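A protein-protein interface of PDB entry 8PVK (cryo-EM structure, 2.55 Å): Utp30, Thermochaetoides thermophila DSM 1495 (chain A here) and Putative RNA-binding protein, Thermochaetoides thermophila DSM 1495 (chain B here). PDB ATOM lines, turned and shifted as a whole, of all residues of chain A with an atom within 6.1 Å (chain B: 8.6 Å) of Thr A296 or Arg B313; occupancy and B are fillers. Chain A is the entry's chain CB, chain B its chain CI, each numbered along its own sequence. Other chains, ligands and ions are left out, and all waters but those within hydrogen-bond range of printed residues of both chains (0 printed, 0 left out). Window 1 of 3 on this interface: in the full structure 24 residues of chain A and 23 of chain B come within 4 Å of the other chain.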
ATOM      1  N   LYS A  69      21.502 -10.253 -41.094  1.00  0.00           N
ATOM      2  CA  LYS A  69      22.672 -11.037 -40.714  1.00  0.00           C
ATOM      3  C   LYS A  69      23.605 -11.249 -41.899  1.00  0.00           C
ATOM      4  O   LYS A  69      24.831 -11.229 -41.742  1.00  0.00           O
ATOM      5  CB  LYS A  69      22.237 -12.378 -40.127  1.00  0.00           C
ATOM      6  CG  LYS A  69      21.547 -12.267 -38.781  1.00  0.00           C
ATOM      7  CD  LYS A  69      20.486 -13.340 -38.630  1.00  0.00           C
ATOM      8  CE  LYS A  69      19.595 -13.074 -37.431  1.00  0.00           C
ATOM      9  NZ  LYS A  69      18.904 -14.310 -36.973  1.00  0.00           N
ATOM     10  N   TRP A 275      12.394 -14.239 -41.560  1.00  0.00           N
ATOM     11  CA  TRP A 275      12.621 -13.519 -40.314  1.00  0.00           C
ATOM     12  C   TRP A 275      13.864 -13.966 -39.557  1.00  0.00           C
ATOM     13  O   TRP A 275      14.316 -13.237 -38.667  1.00  0.00           O
ATOM     14  CB  TRP A 275      11.403 -13.655 -39.394  1.00  0.00           C
ATOM     15  CG  TRP A 275      10.328 -12.652 -39.666  1.00  0.00           C
ATOM     16  CD1 TRP A 275       9.201 -12.840 -40.410  1.00  0.00           C
ATOM     17  CD2 TRP A 275      10.281 -11.300 -39.200  1.00  0.00           C
ATOM     18  NE1 TRP A 275       8.451 -11.689 -40.432  1.00  0.00           N
ATOM     19  CE2 TRP A 275       9.093 -10.727 -39.696  1.00  0.00           C
ATOM     20  CE3 TRP A 275      11.127 -10.517 -38.408  1.00  0.00           C
ATOM     21  CZ2 TRP A 275       8.732  -9.408 -39.430  1.00  0.00           C
ATOM     22  CZ3 TRP A 275      10.765  -9.209 -38.144  1.00  0.00           C
ATOM     23  CH2 TRP A 275       9.579  -8.668 -38.653  1.00  0.00           C
ATOM     24  N   VAL A 278      16.576 -11.366 -40.477  1.00  0.00           N
ATOM     25  CA  VAL A 278      16.437  -9.993 -40.004  1.00  0.00           C
ATOM     26  C   VAL A 278      17.146  -9.843 -38.665  1.00  0.00           C
ATOM     27  O   VAL A 278      16.918 -10.625 -37.733  1.00  0.00           O
ATOM     28  CB  VAL A 278      14.952  -9.614 -39.898  1.00  0.00           C
ATOM     29  CG1 VAL A 278      14.784  -8.269 -39.212  1.00  0.00           C
ATOM     30  CG2 VAL A 278      14.310  -9.600 -41.276  1.00  0.00           C
ATOM     31  N   ARG A 279      18.013  -8.836 -38.563  1.00  0.00           N
ATOM     32  CA  ARG A 279      18.768  -8.579 -37.345  1.00  0.00           C
ATOM     33  C   ARG A 279      18.239  -7.371 -36.580  1.00  0.00           C
ATOM     34  O   ARG A 279      17.914  -7.489 -35.396  1.00  0.00           O
ATOM     35  CB  ARG A 279      20.255  -8.395 -37.678  1.00  0.00           C
ATOM     36  CG  ARG A 279      21.167  -8.308 -36.467  1.00  0.00           C
ATOM     37  CD  ARG A 279      22.549  -7.819 -36.871  1.00  0.00           C
ATOM     38  NE  ARG A 279      23.417  -7.586 -35.724  1.00  0.00           N
ATOM     39  CZ  ARG A 279      24.367  -8.419 -35.320  1.00  0.00           C
ATOM     40  NH1 ARG A 279      24.601  -9.557 -35.952  1.00  0.00           N
ATOM     41  NH2 ARG A 279      25.102  -8.100 -34.260  1.00  0.00           N
ATOM     42  N   ASN A 280      18.142  -6.204 -37.218  1.00  0.00           N
ATOM     43  CA  ASN A 280      17.751  -4.991 -36.512  1.00  0.00           C
ATOM     44  C   ASN A 280      16.872  -4.116 -37.397  1.00  0.00           C
ATOM     45  O   ASN A 280      16.948  -4.158 -38.627  1.00  0.00           O
ATOM     46  CB  ASN A 280      18.971  -4.178 -36.056  1.00  0.00           C
ATOM     47  CG  ASN A 280      19.827  -4.914 -35.045  1.00  0.00           C
ATOM     48  OD1 ASN A 280      20.984  -5.236 -35.312  1.00  0.00           O
ATOM     49  ND2 ASN A 280      19.261  -5.183 -33.875  1.00  0.00           N
ATOM     50  N   TYR A 294      12.906  -3.241 -33.589  1.00  0.00           N
ATOM     51  CA  TYR A 294      12.937  -4.674 -33.312  1.00  0.00           C
ATOM     52  C   TYR A 294      14.380  -5.138 -33.426  1.00  0.00           C
ATOM     53  O   TYR A 294      14.959  -5.109 -34.516  1.00  0.00           O
ATOM     54  CB  TYR A 294      12.037  -5.446 -34.277  1.00  0.00           C
ATOM     55  CG  TYR A 294      12.385  -6.914 -34.393  1.00  0.00           C
ATOM     56  CD1 TYR A 294      12.183  -7.783 -33.327  1.00  0.00           C
ATOM     57  CD2 TYR A 294      12.920  -7.429 -35.567  1.00  0.00           C
ATOM     58  CE1 TYR A 294      12.504  -9.125 -33.429  1.00  0.00           C
ATOM     59  CE2 TYR A 294      13.243  -8.768 -35.678  1.00  0.00           C
ATOM     60  CZ  TYR A 294      13.033  -9.611 -34.607  1.00  0.00           C
ATOM     61  OH  TYR A 294      13.352 -10.945 -34.714  1.00  0.00           O
ATOM     62  N   GLN A 295      14.961  -5.556 -32.307  1.00  0.00           N
ATOM     63  CA  GLN A 295      16.304  -6.117 -32.284  1.00  0.00           C
ATOM     64  C   GLN A 295      16.199  -7.610 -32.008  1.00  0.00           C
ATOM     65  O   GLN A 295      15.473  -8.028 -31.100  1.00  0.00           O
ATOM     66  CB  GLN A 295      17.173  -5.432 -31.228  1.00  0.00           C
ATOM     67  CG  GLN A 295      17.196  -3.914 -31.338  1.00  0.00           C
ATOM     68  CD  GLN A 295      18.528  -3.319 -30.933  1.00  0.00           C
ATOM     69  OE1 GLN A 295      19.581  -3.896 -31.198  1.00  0.00           O
ATOM     70  NE2 GLN A 295      18.491  -2.170 -30.272  1.00  0.00           N
ATOM     71  N   THR A 296      16.916  -8.407 -32.796  1.00  0.00           N
ATOM     72  CA  THR A 296      16.767  -9.852 -32.740  1.00  0.00           C
ATOM     73  C   THR A 296      17.411 -10.418 -31.475  1.00  0.00           C
ATOM     74  O   THR A 296      18.218  -9.770 -30.800  1.00  0.00           O
ATOM     75  CB  THR A 296      17.382 -10.506 -33.977  1.00  0.00           C
ATOM     76  OG1 THR A 296      17.069 -11.905 -33.985  1.00  0.00           O
ATOM     77  CG2 THR A 296      18.895 -10.336 -33.978  1.00  0.00           C
ATOM     78  N   ASP A 297      17.023 -11.650 -31.150  1.00  0.00           N
ATOM     79  CA  ASP A 297      17.591 -12.393 -30.034  1.00  0.00           C
ATOM     80  C   ASP A 297      18.689 -13.353 -30.465  1.00  0.00           C
ATOM     81  O   ASP A 297      19.662 -13.547 -29.730  1.00  0.00           O
ATOM     82  CB  ASP A 297      16.491 -13.173 -29.308  1.00  0.00           C
ATOM     83  CG  ASP A 297      16.920 -13.637 -27.933  1.00  0.00           C
ATOM     84  OD1 ASP A 297      17.343 -12.784 -27.127  1.00  0.00           O
ATOM     85  OD2 ASP A 297      16.834 -14.853 -27.661  1.00  0.00           O
ATOM     86  N   GLU A 298      18.553 -13.954 -31.643  1.00  0.00           N
ATOM     87  CA  GLU A 298      19.553 -14.852 -32.202  1.00  0.00           C
ATOM     88  C   GLU A 298      20.401 -14.080 -33.203  1.00  0.00           C
ATOM     89  O   GLU A 298      19.875 -13.553 -34.189  1.00  0.00           O
ATOM     90  CB  GLU A 298      18.891 -16.052 -32.883  1.00  0.00           C
ATOM     91  CG  GLU A 298      18.003 -16.883 -31.969  1.00  0.00           C
ATOM     92  CD  GLU A 298      17.353 -18.048 -32.689  1.00  0.00           C
ATOM     93  OE1 GLU A 298      17.493 -18.138 -33.927  1.00  0.00           O
ATOM     94  OE2 GLU A 298      16.698 -18.872 -32.016  1.00  0.00           O
ATOM     95  N   LEU A 299      21.705 -14.012 -32.950  1.00  0.00           N
ATOM     96  CA  LEU A 299      22.617 -13.325 -33.854  1.00  0.00           C
ATOM     97  C   LEU A 299      23.229 -14.250 -34.899  1.00  0.00           C
ATOM     98  O   LEU A 299      23.943 -13.769 -35.783  1.00  0.00           O
ATOM     99  CB  LEU A 299      23.731 -12.629 -33.065  1.00  0.00           C
ATOM    100  CG  LEU A 299      23.297 -11.614 -32.008  1.00  0.00           C
ATOM    101  CD1 LEU A 299      24.499 -11.125 -31.207  1.00  0.00           C
ATOM    102  CD2 LEU A 299      22.541 -10.450 -32.640  1.00  0.00           C
ATOM    103  N   VAL B 306      29.105 -11.679 -29.103  1.00  0.00           N
ATOM    104  CA  VAL B 306      27.867 -11.294 -28.440  1.00  0.00           C
ATOM    105  C   VAL B 306      28.148 -10.274 -27.342  1.00  0.00           C
ATOM    106  O   VAL B 306      27.371  -9.336 -27.154  1.00  0.00           O
ATOM    107  CB  VAL B 306      27.111 -12.539 -27.925  1.00  0.00           C
ATOM    108  CG1 VAL B 306      27.810 -13.206 -26.748  1.00  0.00           C
ATOM    109  CG2 VAL B 306      25.687 -12.179 -27.556  1.00  0.00           C
ATOM    110  N   ALA B 307      29.304 -10.379 -26.671  1.00  0.00           N
ATOM    111  CA  ALA B 307      29.622  -9.450 -25.591  1.00  0.00           C
ATOM    112  C   ALA B 307      29.823  -8.038 -26.118  1.00  0.00           C
ATOM    113  O   ALA B 307      29.201  -7.090 -25.612  1.00  0.00           O
ATOM    114  CB  ALA B 307      30.857  -9.920 -24.828  1.00  0.00           C
ATOM    115  N   LYS B 308      30.660  -7.884 -27.161  1.00  0.00           N
ATOM    116  CA  LYS B 308      30.821  -6.564 -27.765  1.00  0.00           C
ATOM    117  C   LYS B 308      29.503  -6.067 -28.334  1.00  0.00           C
ATOM    118  O   LYS B 308      29.255  -4.852 -28.363  1.00  0.00           O
ATOM    119  CB  LYS B 308      31.941  -6.551 -28.825  1.00  0.00           C
ATOM    120  CG  LYS B 308      31.766  -7.405 -30.084  1.00  0.00           C
ATOM    121  CD  LYS B 308      31.078  -6.685 -31.239  1.00  0.00           C
ATOM    122  CE  LYS B 308      31.044  -7.570 -32.469  1.00  0.00           C
ATOM    123  NZ  LYS B 308      30.357  -6.921 -33.614  1.00  0.00           N
ATOM    124  N   GLU B 309      28.618  -6.991 -28.722  1.00  0.00           N
ATOM    125  CA  GLU B 309      27.276  -6.572 -29.086  1.00  0.00           C
ATOM    126  C   GLU B 309      26.509  -5.984 -27.900  1.00  0.00           C
ATOM    127  O   GLU B 309      25.812  -4.982 -28.086  1.00  0.00           O
ATOM    128  CB  GLU B 309      26.493  -7.731 -29.698  1.00  0.00           C
ATOM    129  CG  GLU B 309      25.553  -7.289 -30.796  1.00  0.00           C
ATOM    130  CD  GLU B 309      24.211  -6.823 -30.282  1.00  0.00           C
ATOM    131  OE1 GLU B 309      23.788  -7.285 -29.205  1.00  0.00           O
ATOM    132  OE2 GLU B 309      23.579  -5.982 -30.957  1.00  0.00           O
ATOM    133  N   GLU B 310      26.609  -6.556 -26.680  1.00  0.00           N
ATOM    134  CA  GLU B 310      25.883  -5.875 -25.598  1.00  0.00           C
ATOM    135  C   GLU B 310      26.513  -4.547 -25.197  1.00  0.00           C
ATOM    136  O   GLU B 310      25.766  -3.655 -24.785  1.00  0.00           O
ATOM    137  CB  GLU B 310      25.629  -6.616 -24.259  1.00  0.00           C
ATOM    138  CG  GLU B 310      24.690  -7.822 -24.155  1.00  0.00           C
ATOM    139  CD  GLU B 310      25.305  -9.115 -24.483  1.00  0.00           C
ATOM    140  OE1 GLU B 310      26.511  -9.115 -24.716  1.00  0.00           O
ATOM    141  OE2 GLU B 310      24.577 -10.128 -24.521  1.00  0.00           O
ATOM    142  N   GLN B 311      27.847  -4.366 -25.249  1.00  0.00           N
ATOM    143  CA  GLN B 311      28.190  -2.975 -24.908  1.00  0.00           C
ATOM    144  C   GLN B 311      27.920  -2.017 -26.064  1.00  0.00           C
ATOM    145  O   GLN B 311      27.789  -0.813 -25.818  1.00  0.00           O
ATOM    146  CB  GLN B 311      29.612  -2.658 -24.379  1.00  0.00           C
ATOM    147  CG  GLN B 311      30.880  -2.800 -25.216  1.00  0.00           C
ATOM    148  CD  GLN B 311      31.403  -4.185 -25.325  1.00  0.00           C
ATOM    149  OE1 GLN B 311      30.787  -5.119 -24.855  1.00  0.00           O
ATOM    150  NE2 GLN B 311      32.589  -4.325 -25.907  1.00  0.00           N
ATOM    151  N   ARG B 312      27.764  -2.510 -27.298  1.00  0.00           N
ATOM    152  CA  ARG B 312      27.200  -1.659 -28.344  1.00  0.00           C
ATOM    153  C   ARG B 312      25.750  -1.291 -28.026  1.00  0.00           C
ATOM    154  O   ARG B 312      25.330  -0.138 -28.213  1.00  0.00           O
ATOM    155  CB  ARG B 312      27.307  -2.355 -29.704  1.00  0.00           C
ATOM    156  CG  ARG B 312      26.794  -1.522 -30.869  1.00  0.00           C
ATOM    157  CD  ARG B 312      26.922  -2.260 -32.194  1.00  0.00           C
ATOM    158  NE  ARG B 312      28.317  -2.411 -32.592  1.00  0.00           N
ATOM    159  CZ  ARG B 312      28.736  -3.161 -33.603  1.00  0.00           C
ATOM    160  NH1 ARG B 312      27.888  -3.845 -34.354  1.00  0.00           N
ATOM    161  NH2 ARG B 312      30.038  -3.224 -33.867  1.00  0.00           N
ATOM    162  N   ARG B 313      24.978  -2.261 -27.518  1.00  0.00           N
ATOM    163  CA  ARG B 313      23.613  -1.992 -27.063  1.00  0.00           C
ATOM    164  C   ARG B 313      23.598  -0.971 -25.933  1.00  0.00           C
ATOM    165  O   ARG B 313      22.744  -0.081 -25.903  1.00  0.00           O
ATOM    166  CB  ARG B 313      22.935  -3.281 -26.591  1.00  0.00           C
ATOM    167  CG  ARG B 313      22.742  -4.364 -27.635  1.00  0.00           C
ATOM    168  CD  ARG B 313      21.667  -4.027 -28.646  1.00  0.00           C
ATOM    169  NE  ARG B 313      21.519  -5.099 -29.625  1.00  0.00           N
ATOM    170  CZ  ARG B 313      20.727  -6.151 -29.472  1.00  0.00           C
ATOM    171  NH1 ARG B 313      19.990  -6.310 -28.385  1.00  0.00           N
ATOM    172  NH2 ARG B 313      20.673  -7.068 -30.434  1.00  0.00           N
ATOM    173  N   ALA B 314      24.535  -1.094 -24.992  1.00  0.00           N
ATOM    174  CA  ALA B 314      24.600  -0.174 -23.861  1.00  0.00           C
ATOM    175  C   ALA B 314      25.001   1.229 -24.301  1.00  0.00           C
ATOM    176  O   ALA B 314      24.484   2.221 -23.773  1.00  0.00           O
ATOM    177  CB  ALA B 314      25.572  -0.707 -22.809  1.00  0.00           C
ATOM    178  N   ALA B 315      25.931   1.332 -25.257  1.00  0.00           N
ATOM    179  CA  ALA B 315      26.301   2.635 -25.802  1.00  0.00           C
ATOM    180  C   ALA B 315      25.123   3.288 -26.515  1.00  0.00           C
ATOM    181  O   ALA B 315      24.869   4.487 -26.343  1.00  0.00           O
ATOM    182  CB  ALA B 315      27.492   2.491 -26.748  1.00  0.00           C
ATOM    183  N   ARG B 316      24.375   2.510 -27.301  1.00  0.00           N
ATOM    184  CA  ARG B 316      23.192   3.069 -27.949  1.00  0.00           C
ATOM    185  C   ARG B 316      22.106   3.421 -26.938  1.00  0.00           C
ATOM    186  O   ARG B 316      21.382   4.402 -27.128  1.00  0.00           O
ATOM    187  CB  ARG B 316      22.667   2.102 -29.011  1.00  0.00           C
ATOM    188  CG  ARG B 316      23.427   2.212 -30.326  1.00  0.00           C
ATOM    189  CD  ARG B 316      22.900   1.261 -31.383  1.00  0.00           C
ATOM    190  NE  ARG B 316      23.293  -0.117 -31.119  1.00  0.00           N
ATOM    191  CZ  ARG B 316      22.977  -1.146 -31.892  1.00  0.00           C
ATOM    192  NH1 ARG B 316      22.264  -0.986 -32.994  1.00  0.00           N
ATOM    193  NH2 ARG B 316      23.390  -2.364 -31.555  1.00  0.00           N
ATOM    194  N   ALA B 317      22.003   2.665 -25.841  1.00  0.00           N
ATOM    195  CA  ALA B 317      21.027   2.985 -24.802  1.00  0.00           C
ATOM    196  C   ALA B 317      21.377   4.282 -24.081  1.00  0.00           C
ATOM    197  O   ALA B 317      20.495   5.111 -23.821  1.00  0.00           O
ATOM    198  CB  ALA B 317      20.924   1.829 -23.807  1.00  0.00           C
ATOM    199  N   GLU B 318      22.653   4.484 -23.749  1.00  0.00           N
ATOM    200  CA  GLU B 318      23.035   5.740 -23.115  1.00  0.00           C
ATOM    201  C   GLU B 318      23.017   6.911 -24.090  1.00  0.00           C
ATOM    202  O   GLU B 318      22.918   8.060 -23.645  1.00  0.00           O
ATOM    203  CB  GLU B 318      24.405   5.615 -22.428  1.00  0.00           C
ATOM    204  CG  GLU B 318      25.599   5.282 -23.314  1.00  0.00           C
ATOM    205  CD  GLU B 318      26.238   6.503 -23.951  1.00  0.00           C
ATOM    206  OE1 GLU B 318      26.022   7.622 -23.443  1.00  0.00           O
ATOM    207  OE2 GLU B 318      26.957   6.339 -24.959  1.00  0.00           O
ATOM    208  N   LYS B 319      23.107   6.654 -25.399  1.00  0.00           N
ATOM    209  CA  LYS B 319      22.808   7.707 -26.364  1.00  0.00           C
ATOM    210  C   LYS B 319      21.311   7.987 -26.444  1.00  0.00           C
ATOM    211  O   LYS B 319      20.907   9.120 -26.728  1.00  0.00           O
ATOM    212  CB  LYS B 319      23.352   7.336 -27.744  1.00  0.00           C
ATOM    213  CG  LYS B 319      24.867   7.382 -27.849  1.00  0.00           C
ATOM    214  CD  LYS B 319      25.384   8.804 -27.712  1.00  0.00           C
ATOM    215  CE  LYS B 319      25.062   9.626 -28.948  1.00  0.00           C
ATOM    216  NZ  LYS B 319      25.642  10.995 -28.871  1.00  0.00           N
ATOM    217  N   LEU B 320      20.478   6.973 -26.211  1.00  0.00           N
ATOM    218  CA  LEU B 320      19.030   7.150 -26.226  1.00  0.00           C
ATOM    219  C   LEU B 320      18.481   7.735 -24.932  1.00  0.00           C
ATOM    220  O   LEU B 320      17.301   8.103 -24.898  1.00  0.00           O
ATOM    221  CB  LEU B 320      18.335   5.816 -26.505  1.00  0.00           C
ATOM    222  CG  LEU B 320      18.361   5.290 -27.940  1.00  0.00           C
ATOM    223  CD1 LEU B 320      17.946   3.829 -27.968  1.00  0.00           C
ATOM    224  CD2 LEU B 320      17.464   6.123 -28.832  1.00  0.00           C
ATOM    225  N   LYS B 321      19.288   7.780 -23.866  1.00  0.00           N
ATOM    226  CA  LYS B 321      18.822   8.343 -22.597  1.00  0.00           C
ATOM    227  C   LYS B 321      18.423   9.810 -22.741  1.00  0.00           C
ATOM    228  O   LYS B 321      17.331  10.208 -22.318  1.00  0.00           O
ATOM    229  CB  LYS B 321      19.894   8.191 -21.516  1.00  0.00           C
ATOM    230  CG  LYS B 321      20.156   6.763 -21.056  1.00  0.00           C
ATOM    231  CD  LYS B 321      18.956   6.152 -20.345  1.00  0.00           C
ATOM    232  CE  LYS B 321      18.392   4.972 -21.123  1.00  0.00           C
ATOM    233  NZ  LYS B 321      17.403   4.195 -20.326  1.00  0.00           N
ATOM    234  N   PHE B 327      14.014   2.065 -24.912  1.00  0.00           N
ATOM    235  CA  PHE B 327      13.830   0.792 -25.596  1.00  0.00           C
ATOM    236  C   PHE B 327      14.313  -0.339 -24.704  1.00  0.00           C
ATOM    237  O   PHE B 327      15.431  -0.289 -24.180  1.00  0.00           O
ATOM    238  CB  PHE B 327      14.578   0.754 -26.931  1.00  0.00           C
ATOM    239  CG  PHE B 327      14.159  -0.383 -27.824  1.00  0.00           C
ATOM    240  CD1 PHE B 327      15.083  -1.329 -28.238  1.00  0.00           C
ATOM    241  CD2 PHE B 327      12.843  -0.513 -28.235  1.00  0.00           C
ATOM    242  CE1 PHE B 327      14.705  -2.379 -29.054  1.00  0.00           C
ATOM    243  CE2 PHE B 327      12.457  -1.562 -29.051  1.00  0.00           C
ATOM    244  CZ  PHE B 327      13.390  -2.496 -29.461  1.00  0.00           C
ATOM    245  N   GLU B 328      13.473  -1.355 -24.536  1.00  0.00           N
ATOM    246  CA  GLU B 328      13.857  -2.553 -23.806  1.00  0.00           C
ATOM    247  C   GLU B 328      14.538  -3.533 -24.753  1.00  0.00           C
ATOM    248  O   GLU B 328      14.240  -3.572 -25.951  1.00  0.00           O
ATOM    249  CB  GLU B 328      12.640  -3.206 -23.142  1.00  0.00           C
ATOM    250  CG  GLU B 328      11.593  -3.763 -24.101  1.00  0.00           C
ATOM    251  CD  GLU B 328      10.530  -2.747 -24.479  1.00  0.00           C
ATOM    252  OE1 GLU B 328      10.739  -1.540 -24.238  1.00  0.00           O
ATOM    253  OE2 GLU B 328       9.483  -3.159 -25.019  1.00  0.00           O
ATOM    254  N   ALA B 329      15.475  -4.303 -24.214  1.00  0.00           N
ATOM    255  CA  ALA B 329      16.192  -5.270 -25.025  1.00  0.00           C
ATOM    256  C   ALA B 329      15.973  -6.679 -24.493  1.00  0.00           C
ATOM    257  O   ALA B 329      16.062  -6.901 -23.280  1.00  0.00           O
ATOM    258  CB  ALA B 329      17.695  -4.966 -25.049  1.00  0.00           C
ATOM    259  N   PRO B 330      15.665  -7.638 -25.364  1.00  0.00           N
ATOM    260  CA  PRO B 330      15.522  -9.025 -24.913  1.00  0.00           C
ATOM    261  C   PRO B 330      16.849  -9.594 -24.438  1.00  0.00           C
ATOM    262  O   PRO B 330      17.923  -9.202 -24.902  1.00  0.00           O
ATOM    263  CB  PRO B 330      15.019  -9.759 -26.163  1.00  0.00           C
ATOM    264  CG  PRO B 330      14.489  -8.683 -27.063  1.00  0.00           C
ATOM    265  CD  PRO B 330      15.342  -7.486 -26.792  1.00  0.00           C
ATOM    266  N   ALA B 331      16.761 -10.525 -23.491  1.00  0.00           N
ATOM    267  CA  ALA B 331      17.946 -11.174 -22.940  1.00  0.00           C
ATOM    268  C   ALA B 331      18.568 -12.072 -24.001  1.00  0.00           C
ATOM    269  O   ALA B 331      18.011 -13.121 -24.340  1.00  0.00           O
ATOM    270  CB  ALA B 331      17.582 -11.970 -21.692  1.00  0.00           C
ATOM    271  N   LEU B 332      19.719 -11.658 -24.525  1.00  0.00           N
ATOM    272  CA  LEU B 332      20.374 -12.396 -25.597  1.00  0.00           C
ATOM    273  C   LEU B 332      20.922 -13.717 -25.075  1.00  0.00           C
ATOM    274  O   LEU B 332      21.756 -13.742 -24.164  1.00  0.00           O
ATOM    275  CB  LEU B 332      21.497 -11.556 -26.200  1.00  0.00           C
ATOM    276  CG  LEU B 332      21.072 -10.226 -26.822  1.00  0.00           C
ATOM    277  CD1 LEU B 332      22.294  -9.412 -27.198  1.00  0.00           C
ATOM    278  CD2 LEU B 332      20.180 -10.449 -28.034  1.00  0.00           C
ATOM    279  N   LYS B 333      20.451 -14.816 -25.658  1.00  0.00           N
ATOM    280  CA  LYS B 333      20.827 -16.141 -25.185  1.00  0.00           C
ATOM    281  C   LYS B 333      22.154 -16.576 -25.798  1.00  0.00           C
ATOM    282  O   LYS B 333      22.484 -16.209 -26.930  1.00  0.00           O
ATOM    283  CB  LYS B 333      19.716 -17.145 -25.500  1.00  0.00           C
ATOM    284  CG  LYS B 333      19.484 -17.423 -26.980  1.00  0.00           C
ATOM    285  CD  LYS B 333      18.335 -18.406 -27.171  1.00  0.00           C
ATOM    286  CE  LYS B 333      18.048 -18.669 -28.642  1.00  0.00           C
ATOM    287  NZ  LYS B 333      19.167 -19.392 -29.303  1.00  0.00           N
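The backbone carbonyl oxygen (O) of Ala B331 lies close to the side-chain carboxylate (OD1) of Asp A297 (2.9 Å). The side-chain carboxylate (OE2) of Glu A298 lies within salt-bridge range of the side-chain amino group (NZ) of Lys B333 (3.7 Å). The side-chain amide oxygen (OE1) of Gln A295 is in hydrogen-bond range of the guanidinium group (NE) of Arg B313 (2.8 Å).
Thr A296 touches just these residues of chain B: Arg B313 (3.7 Å) and Leu B332 (3.5 Å). Printed residues of chain B within 4 Å of Asp A297: Pro B330 (3.9 Å), Ala B331 (2.9 Å), Leu B332 (3.4 Å) and Lys B333 (3.8 Å). Printed residues of chain B within 4 Å of Glu A298: Lys B333. Of the printed residues of chain B, Leu A299 touches Val B306 and Glu B309. Of chain A, only Gln A295 and Thr A296 come within 4 Å of Arg B313. Ala B315 touches none of the printed residues of chain A. Lys B319 touches none of the printed residues of chain A. Of the printed residues of chain A, Pro B330 touches Asp A297 (3.9 Å). Of the printed residues of chain A, Ala B331 touches Asp A297 (2.9 Å). The nearest printed residue of chain A that does not touch Lys B333 is Leu A299 (6.5 Å).
The side-chain amino group (NZ) of Lys A69 lies within hydrogen-bond range of the backbone carbonyl oxygen (O) of Glu A298. The side-chain carboxylate (OE2) of Glu B309 is in salt-bridge range of the guanidinium group (NH2) of Arg B316 (3.7 Å). The backbone carbonyl oxygen (O) of Val B306 sits close to the side-chain carboxylate (OE1) of Glu B310. The guanidinium group (NE) of Arg B313 lies within salt-bridge range of the side-chain carboxylate (OE2) of Glu B309. OE1 of Gln A295 sits at hydrogen-bond distance from ND2 of Asn A280 (3.0 Å). O of Arg A279 sits at hydrogen-bond distance from N of Thr A296 (2.9 Å).
Among the printed residues, merely in contact across the chains: Arg A279 with Glu B309, Gln A295 with Phe B327, Thr A296 with Arg B313, Thr A296 with Leu B332, Asp A297 with Pro B330, Asp A297 with Leu B332, Asp A297 with Lys B333, Leu A299 with Val B306 and Leu A299 with Glu B309.
Hydrophobic or aromatic side chains of chain A that line the printed part of chain B: Leu A299. Of the 23 printed residues of chain B, 8 touch a printed residue of chain A. Among the printed residues, Asp or Glu carboxylates within 4 Å of a Lys or Arg side-chain nitrogen of the other chain: Glu A298 with Lys B333.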
